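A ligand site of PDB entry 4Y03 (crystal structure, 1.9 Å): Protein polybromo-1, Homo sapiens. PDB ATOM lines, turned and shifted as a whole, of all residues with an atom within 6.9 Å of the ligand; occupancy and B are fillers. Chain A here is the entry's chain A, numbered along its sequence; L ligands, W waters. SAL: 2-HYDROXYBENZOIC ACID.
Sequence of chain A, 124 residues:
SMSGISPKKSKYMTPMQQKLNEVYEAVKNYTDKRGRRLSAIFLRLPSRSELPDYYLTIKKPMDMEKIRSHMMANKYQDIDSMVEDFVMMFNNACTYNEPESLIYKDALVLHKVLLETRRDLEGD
The side-chain hydroxyl of Tyr 54 is in hydrogen-bond range of an oxygen (O2) of the ligand (2.8 Å).
ND2 of Asn 97 lies within hydrogen-bond range of O1' of the ligand (3.0 Å).
The backbone NH of Ala 93 lies close to an oxygen (O2) of the ligand, at 3.3 Å.
The side-chain amide nitrogen of Asn 97 sits at hydrogen-bond distance from the backbone carbonyl oxygen of Ala 93 (2.6 Å).
The backbone NH of Leu 45 is in hydrogen-bond range of the side-chain carboxylate of Asp 63, at 3.0 Å.
The backbone carbonyl oxygen (O) of Phe 42 lies within hydrogen-bond range of the backbone NH (N) of Met 64, 2.9 Å away.
The side-chain amide oxygen of Asn 92 lies close to the backbone carbonyl oxygen of Met 88 (3.3 Å).
The side-chain sulfur (SD) of Met 89 lies close to the backbone NH (N) of Met 64 (3.8 Å).
Ile 41 touches the ligand (O to C6, 3.3 Å).
Phe 42 touches the ligand.
Leu 45 touches the ligand.
Met 62 touches the ligand.
Met 89 touches the ligand (CG to C4, 3.96 Å).
C of Asn 92 touches O2 of the ligand, at 3.9 Å.
Ile 103 touches the ligand (CG2 to O1', 3.8 Å).
Hydrophobic or aromatic side chains within 4 Å of the ligand: Ile 41, Phe 42, Leu 45, Tyr 54, Met 89, Ala 93 and Ile 103.
Of the 23 residues printed, 10 come within 4 Å of the ligand.
The nearest printed residue that does not touch the ligand is Asp 63 (4.3 Å).
Water W1 lies within hydrogen-bond range of an oxygen (O1') of the ligand and the side-chain amide oxygen (OD1) of Asn 97.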
ATOM      1  N   ILE A  41     -14.360  -9.604 -19.061  1.00  0.00           N
ATOM      2  CA  ILE A  41     -15.596  -8.854 -19.266  1.00  0.00           C
ATOM      3  C   ILE A  41     -15.271  -7.430 -19.714  1.00  0.00           C
ATOM      4  O   ILE A  41     -16.123  -6.739 -20.236  1.00  0.00           O
ATOM      5  CB  ILE A  41     -16.515  -8.896 -17.976  1.00  0.00           C
ATOM      6  CG1 ILE A  41     -17.977  -8.673 -18.343  1.00  0.00           C
ATOM      7  CG2 ILE A  41     -16.118  -7.812 -16.931  1.00  0.00           C
ATOM      8  CD1 ILE A  41     -18.896  -8.627 -17.146  1.00  0.00           C
ATOM      9  N   PHE A  42     -14.005  -7.003 -19.563  1.00  0.00           N
ATOM     10  CA  PHE A  42     -13.611  -5.652 -19.896  1.00  0.00           C
ATOM     11  C   PHE A  42     -13.147  -5.488 -21.336  1.00  0.00           C
ATOM     12  O   PHE A  42     -12.921  -4.382 -21.803  1.00  0.00           O
ATOM     13  CB  PHE A  42     -12.500  -5.211 -18.945  1.00  0.00           C
ATOM     14  CG  PHE A  42     -12.950  -5.143 -17.505  1.00  0.00           C
ATOM     15  CD1 PHE A  42     -13.733  -4.095 -17.066  1.00  0.00           C
ATOM     16  CD2 PHE A  42     -12.627  -6.167 -16.606  1.00  0.00           C
ATOM     17  CE1 PHE A  42     -14.189  -4.044 -15.746  1.00  0.00           C
ATOM     18  CE2 PHE A  42     -13.053  -6.098 -15.285  1.00  0.00           C
ATOM     19  CZ  PHE A  42     -13.832  -5.033 -14.863  1.00  0.00           C
ATOM     20  N   LEU A  43     -12.959  -6.581 -22.060  1.00  0.00           N
ATOM     21  CA  LEU A  43     -12.373  -6.476 -23.389  1.00  0.00           C
ATOM     22  C   LEU A  43     -13.305  -5.700 -24.296  1.00  0.00           C
ATOM     23  O   LEU A  43     -12.859  -4.888 -25.142  1.00  0.00           O
ATOM     24  CB  LEU A  43     -12.081  -7.866 -23.973  1.00  0.00           C
ATOM     25  CG  LEU A  43     -11.236  -8.759 -23.028  1.00  0.00           C
ATOM     26  CD1 LEU A  43     -11.191 -10.243 -23.405  1.00  0.00           C
ATOM     27  CD2 LEU A  43      -9.818  -8.214 -22.863  1.00  0.00           C
ATOM     28  N   ARG A  44     -14.604  -5.971 -24.165  1.00  0.00           N
ATOM     29  CA  ARG A  44     -15.581  -5.376 -25.028  1.00  0.00           C
ATOM     30  C   ARG A  44     -16.947  -5.176 -24.368  1.00  0.00           C
ATOM     31  O   ARG A  44     -17.609  -6.111 -23.905  1.00  0.00           O
ATOM     32  CB  ARG A  44     -15.648  -6.218 -26.316  1.00  0.00           C
ATOM     33  CG  ARG A  44     -16.821  -5.968 -27.184  1.00  0.00           C
ATOM     34  CD  ARG A  44     -17.016  -4.525 -27.549  1.00  0.00           C
ATOM     35  NE  ARG A  44     -16.475  -4.177 -28.857  1.00  0.00           N
ATOM     36  CZ  ARG A  44     -16.718  -3.019 -29.471  1.00  0.00           C
ATOM     37  NH1 ARG A  44     -17.475  -2.096 -28.893  1.00  0.00           N
ATOM     38  NH2 ARG A  44     -16.190  -2.786 -30.661  1.00  0.00           N
ATOM     39  N   LEU A  45     -17.341  -3.904 -24.254  1.00  0.00           N
ATOM     40  CA  LEU A  45     -18.582  -3.526 -23.600  1.00  0.00           C
ATOM     41  C   LEU A  45     -19.741  -3.917 -24.529  1.00  0.00           C
ATOM     42  O   LEU A  45     -19.623  -3.814 -25.750  1.00  0.00           O
ATOM     43  CB  LEU A  45     -18.568  -2.012 -23.321  1.00  0.00           C
ATOM     44  CG  LEU A  45     -19.644  -1.438 -22.389  1.00  0.00           C
ATOM     45  CD1 LEU A  45     -19.564  -2.022 -20.964  1.00  0.00           C
ATOM     46  CD2 LEU A  45     -19.570   0.103 -22.360  1.00  0.00           C
ATOM     47  N   PRO A  46     -20.845  -4.441 -23.964  1.00  0.00           N
ATOM     48  CA  PRO A  46     -21.947  -4.735 -24.880  1.00  0.00           C
ATOM     49  C   PRO A  46     -22.612  -3.493 -25.453  1.00  0.00           C
ATOM     50  O   PRO A  46     -22.204  -2.346 -25.153  1.00  0.00           O
ATOM     51  CB  PRO A  46     -22.927  -5.545 -24.016  1.00  0.00           C
ATOM     52  CG  PRO A  46     -22.081  -6.089 -22.904  1.00  0.00           C
ATOM     53  CD  PRO A  46     -21.033  -5.061 -22.647  1.00  0.00           C
ATOM     54  N   LEU A  51     -27.492  -3.247 -23.104  1.00  0.00           N
ATOM     55  CA  LEU A  51     -27.350  -2.633 -21.785  1.00  0.00           C
ATOM     56  C   LEU A  51     -27.956  -1.216 -21.743  1.00  0.00           C
ATOM     57  O   LEU A  51     -27.220  -0.226 -21.635  1.00  0.00           O
ATOM     58  CB  LEU A  51     -25.872  -2.607 -21.370  1.00  0.00           C
ATOM     59  CG  LEU A  51     -25.173  -3.922 -20.983  1.00  0.00           C
ATOM     60  CD1 LEU A  51     -23.685  -3.627 -20.667  1.00  0.00           C
ATOM     61  CD2 LEU A  51     -25.866  -4.600 -19.829  1.00  0.00           C
ATOM     62  N   TYR A  54     -26.958   0.978 -18.764  1.00  0.00           N
ATOM     63  CA  TYR A  54     -25.532   1.320 -18.731  1.00  0.00           C
ATOM     64  C   TYR A  54     -25.226   2.616 -19.435  1.00  0.00           C
ATOM     65  O   TYR A  54     -24.640   3.548 -18.867  1.00  0.00           O
ATOM     66  CB  TYR A  54     -24.679   0.196 -19.358  1.00  0.00           C
ATOM     67  CG  TYR A  54     -23.194   0.322 -19.081  1.00  0.00           C
ATOM     68  CD1 TYR A  54     -22.390   1.212 -19.815  1.00  0.00           C
ATOM     69  CD2 TYR A  54     -22.589  -0.411 -18.064  1.00  0.00           C
ATOM     70  CE1 TYR A  54     -21.045   1.364 -19.545  1.00  0.00           C
ATOM     71  CE2 TYR A  54     -21.230  -0.270 -17.790  1.00  0.00           C
ATOM     72  CZ  TYR A  54     -20.467   0.621 -18.544  1.00  0.00           C
ATOM     73  OH  TYR A  54     -19.137   0.791 -18.301  1.00  0.00           O
ATOM     74  N   ILE A  58     -23.535   5.971 -17.853  1.00  0.00           N
ATOM     75  CA  ILE A  58     -22.108   6.178 -18.116  1.00  0.00           C
ATOM     76  C   ILE A  58     -21.909   7.256 -19.217  1.00  0.00           C
ATOM     77  O   ILE A  58     -22.320   7.115 -20.358  1.00  0.00           O
ATOM     78  CB  ILE A  58     -21.413   4.833 -18.432  1.00  0.00           C
ATOM     79  CG1 ILE A  58     -21.719   3.839 -17.329  1.00  0.00           C
ATOM     80  CG2 ILE A  58     -19.858   4.981 -18.575  1.00  0.00           C
ATOM     81  CD1 ILE A  58     -21.410   4.316 -15.916  1.00  0.00           C
ATOM     82  N   PRO A  61     -18.253   5.824 -22.209  1.00  0.00           N
ATOM     83  CA  PRO A  61     -18.048   4.380 -22.117  1.00  0.00           C
ATOM     84  C   PRO A  61     -16.643   3.948 -22.591  1.00  0.00           C
ATOM     85  O   PRO A  61     -16.069   4.574 -23.499  1.00  0.00           O
ATOM     86  CB  PRO A  61     -19.156   3.837 -23.001  1.00  0.00           C
ATOM     87  CG  PRO A  61     -20.290   4.913 -22.849  1.00  0.00           C
ATOM     88  CD  PRO A  61     -19.494   6.162 -22.942  1.00  0.00           C
ATOM     89  N   MET A  62     -16.082   2.919 -21.964  1.00  0.00           N
ATOM     90  CA  MET A  62     -14.695   2.507 -22.248  1.00  0.00           C
ATOM     91  C   MET A  62     -14.511   1.003 -22.098  1.00  0.00           C
ATOM     92  O   MET A  62     -15.074   0.393 -21.213  1.00  0.00           O
ATOM     93  CB  MET A  62     -13.717   3.289 -21.354  1.00  0.00           C
ATOM     94  CG  MET A  62     -12.174   3.049 -21.668  1.00  0.00           C
ATOM     95  SD  MET A  62     -11.659   3.546 -23.357  1.00  0.00           S
ATOM     96  CE  MET A  62     -11.970   5.312 -23.348  1.00  0.00           C
ATOM     97  N   ASP A  63     -13.753   0.405 -23.025  1.00  0.00           N
ATOM     98  CA  ASP A  63     -13.371  -1.002 -22.894  1.00  0.00           C
ATOM     99  C   ASP A  63     -11.945  -1.189 -23.412  1.00  0.00           C
ATOM    100  O   ASP A  63     -11.390  -0.269 -23.994  1.00  0.00           O
ATOM    101  CB  ASP A  63     -14.373  -1.907 -23.598  1.00  0.00           C
ATOM    102  CG  ASP A  63     -14.527  -1.611 -25.102  1.00  0.00           C
ATOM    103  OD1 ASP A  63     -13.611  -1.078 -25.749  1.00  0.00           O
ATOM    104  OD2 ASP A  63     -15.602  -1.953 -25.631  1.00  0.00           O
ATOM    105  N   MET A  64     -11.364  -2.366 -23.221  1.00  0.00           N
ATOM    106  CA  MET A  64      -9.950  -2.588 -23.575  1.00  0.00           C
ATOM    107  C   MET A  64      -9.710  -2.610 -25.071  1.00  0.00           C
ATOM    108  O   MET A  64      -8.608  -2.300 -25.508  1.00  0.00           O
ATOM    109  CB  MET A  64      -9.435  -3.831 -22.913  1.00  0.00           C
ATOM    110  CG  MET A  64      -9.388  -3.597 -21.421  1.00  0.00           C
ATOM    111  SD  MET A  64      -8.704  -4.891 -20.419  1.00  0.00           S
ATOM    112  CE  MET A  64      -7.091  -5.085 -21.193  1.00  0.00           C
ATOM    113  N   MET A  88     -10.695   5.438 -16.493  1.00  0.00           N
ATOM    114  CA  MET A  88     -12.091   5.733 -16.877  1.00  0.00           C
ATOM    115  C   MET A  88     -12.915   4.446 -16.862  1.00  0.00           C
ATOM    116  O   MET A  88     -14.033   4.390 -16.302  1.00  0.00           O
ATOM    117  CB  MET A  88     -12.147   6.423 -18.251  1.00  0.00           C
ATOM    118  CG  MET A  88     -13.528   6.852 -18.756  1.00  0.00           C
ATOM    119  SD  MET A  88     -14.480   7.970 -17.685  1.00  0.00           S
ATOM    120  CE  MET A  88     -13.472   9.512 -17.769  1.00  0.00           C
ATOM    121  N   MET A  89     -12.320   3.385 -17.395  1.00  0.00           N
ATOM    122  CA  MET A  89     -13.016   2.114 -17.517  1.00  0.00           C
ATOM    123  C   MET A  89     -13.348   1.547 -16.155  1.00  0.00           C
ATOM    124  O   MET A  89     -14.507   1.071 -15.930  1.00  0.00           O
ATOM    125  CB  MET A  89     -12.169   1.129 -18.312  1.00  0.00           C
ATOM    126  CG  MET A  89     -12.861  -0.180 -18.688  1.00  0.00           C
ATOM    127  SD  MET A  89     -11.738  -1.256 -19.614  1.00  0.00           S
ATOM    128  CE  MET A  89     -10.604  -1.704 -18.250  1.00  0.00           C
ATOM    129  N   PHE A  90     -12.369   1.590 -15.243  1.00  0.00           N
ATOM    130  CA  PHE A  90     -12.566   0.996 -13.895  1.00  0.00           C
ATOM    131  C   PHE A  90     -13.497   1.872 -13.079  1.00  0.00           C
ATOM    132  O   PHE A  90     -14.312   1.363 -12.321  1.00  0.00           O
ATOM    133  CB  PHE A  90     -11.270   0.747 -13.134  1.00  0.00           C
ATOM    134  CG  PHE A  90     -10.275  -0.104 -13.874  1.00  0.00           C
ATOM    135  CD1 PHE A  90     -10.642  -1.320 -14.404  1.00  0.00           C
ATOM    136  CD2 PHE A  90      -8.945   0.298 -13.986  1.00  0.00           C
ATOM    137  CE1 PHE A  90      -9.738  -2.099 -15.066  1.00  0.00           C
ATOM    138  CE2 PHE A  90      -8.043  -0.479 -14.634  1.00  0.00           C
ATOM    139  CZ  PHE A  90      -8.436  -1.694 -15.182  1.00  0.00           C
ATOM    140  N   ASN A  91     -13.357   3.179 -13.213  1.00  0.00           N
ATOM    141  CA  ASN A  91     -14.382   4.085 -12.681  1.00  0.00           C
ATOM    142  C   ASN A  91     -15.791   3.781 -13.209  1.00  0.00           C
ATOM    143  O   ASN A  91     -16.733   3.787 -12.435  1.00  0.00           O
ATOM    144  CB  ASN A  91     -14.033   5.567 -12.911  1.00  0.00           C
ATOM    145  CG  ASN A  91     -13.181   6.124 -11.781  1.00  0.00           C
ATOM    146  OD1 ASN A  91     -13.432   5.848 -10.599  1.00  0.00           O
ATOM    147  ND2 ASN A  91     -12.170   6.915 -12.125  1.00  0.00           N
ATOM    148  N   ASN A  92     -15.921   3.505 -14.495  1.00  0.00           N
ATOM    149  CA  ASN A  92     -17.232   3.244 -15.074  1.00  0.00           C
ATOM    150  C   ASN A  92     -17.821   1.973 -14.483  1.00  0.00           C
ATOM    151  O   ASN A  92     -18.980   1.963 -14.059  1.00  0.00           O
ATOM    152  CB  ASN A  92     -17.176   3.114 -16.613  1.00  0.00           C
ATOM    153  CG  ASN A  92     -16.925   4.425 -17.326  1.00  0.00           C
ATOM    154  OD1 ASN A  92     -17.048   5.520 -16.752  1.00  0.00           O
ATOM    155  ND2 ASN A  92     -16.541   4.324 -18.625  1.00  0.00           N
ATOM    156  N   ALA A  93     -17.023   0.914 -14.428  1.00  0.00           N
ATOM    157  CA  ALA A  93     -17.453  -0.389 -13.869  1.00  0.00           C
ATOM    158  C   ALA A  93     -17.870  -0.342 -12.414  1.00  0.00           C
ATOM    159  O   ALA A  93     -18.781  -1.082 -11.985  1.00  0.00           O
ATOM    160  CB  ALA A  93     -16.362  -1.422 -14.040  1.00  0.00           C
ATOM    161  N   CYS A  94     -17.157   0.482 -11.647  1.00  0.00           N
ATOM    162  CA  CYS A  94     -17.449   0.649 -10.246  1.00  0.00           C
ATOM    163  C   CYS A  94     -18.664   1.538 -10.045  1.00  0.00           C
ATOM    164  O   CYS A  94     -19.475   1.260  -9.166  1.00  0.00           O
ATOM    165  CB  CYS A  94     -16.240   1.189  -9.515  1.00  0.00           C
ATOM    166  SG  CYS A  94     -14.917  -0.151  -9.304  1.00  0.00           S
ATOM    167  N   TYR A  96     -21.309   1.711 -12.164  1.00  0.00           N
ATOM    168  CA  TYR A  96     -22.532   1.025 -12.585  1.00  0.00           C
ATOM    169  C   TYR A  96     -22.870  -0.124 -11.664  1.00  0.00           C
ATOM    170  O   TYR A  96     -24.043  -0.368 -11.391  1.00  0.00           O
ATOM    171  CB  TYR A  96     -22.408   0.514 -14.039  1.00  0.00           C
ATOM    172  CG  TYR A  96     -23.631  -0.223 -14.596  1.00  0.00           C
ATOM    173  CD1 TYR A  96     -24.763   0.476 -15.004  1.00  0.00           C
ATOM    174  CD2 TYR A  96     -23.622  -1.621 -14.760  1.00  0.00           C
ATOM    175  CE1 TYR A  96     -25.884  -0.196 -15.529  1.00  0.00           C
ATOM    176  CE2 TYR A  96     -24.753  -2.311 -15.276  1.00  0.00           C
ATOM    177  CZ  TYR A  96     -25.864  -1.581 -15.665  1.00  0.00           C
ATOM    178  OH  TYR A  96     -26.969  -2.222 -16.179  1.00  0.00           O
ATOM    179  N   ASN A  97     -21.825  -0.801 -11.176  1.00  0.00           N
ATOM    180  CA  ASN A  97     -22.002  -2.055 -10.499  1.00  0.00           C
ATOM    181  C   ASN A  97     -21.945  -1.819  -8.978  1.00  0.00           C
ATOM    182  O   ASN A  97     -21.456  -0.768  -8.507  1.00  0.00           O
ATOM    183  CB  ASN A  97     -20.972  -3.080 -10.939  1.00  0.00           C
ATOM    184  CG  ASN A  97     -21.087  -3.453 -12.395  1.00  0.00           C
ATOM    185  OD1 ASN A  97     -21.960  -4.232 -12.764  1.00  0.00           O
ATOM    186  ND2 ASN A  97     -20.187  -2.925 -13.232  1.00  0.00           N
ATOM    187  N   ILE A 103     -17.720  -7.722 -10.602  1.00  0.00           N
ATOM    188  CA  ILE A 103     -17.143  -6.859 -11.627  1.00  0.00           C
ATOM    189  C   ILE A 103     -16.412  -5.748 -10.904  1.00  0.00           C
ATOM    190  O   ILE A 103     -15.275  -5.399 -11.256  1.00  0.00           O
ATOM    191  CB  ILE A 103     -18.217  -6.265 -12.567  1.00  0.00           C
ATOM    192  CG1 ILE A 103     -18.861  -7.356 -13.434  1.00  0.00           C
ATOM    193  CG2 ILE A 103     -17.646  -5.121 -13.414  1.00  0.00           C
ATOM    194  CD1 ILE A 103     -17.969  -8.519 -13.812  1.00  0.00           C
HETATM  195  C1' SAL L   1     -19.267  -3.941 -17.239  1.00  0.00           C
HETATM  196  O1' SAL L   1     -19.557  -3.393 -16.152  1.00  0.00           O
HETATM  197  O2' SAL L   1     -19.816  -4.985 -17.639  1.00  0.00           O
HETATM  198  C1  SAL L   1     -18.153  -3.298 -18.096  1.00  0.00           C
HETATM  199  C2  SAL L   1     -17.628  -2.019 -17.780  1.00  0.00           C
HETATM  200  C3  SAL L   1     -16.611  -1.501 -18.592  1.00  0.00           C
HETATM  201  C4  SAL L   1     -16.107  -2.226 -19.682  1.00  0.00           C
HETATM  202  C5  SAL L   1     -16.625  -3.494 -19.992  1.00  0.00           C
HETATM  203  C6  SAL L   1     -17.634  -4.026 -19.197  1.00  0.00           C
HETATM  204  O2  SAL L   1     -18.101  -1.253 -16.729  1.00  0.00           O
HETATM  205  O   HOH W   1     -22.302  -4.631 -15.963  1.00  0.00           O
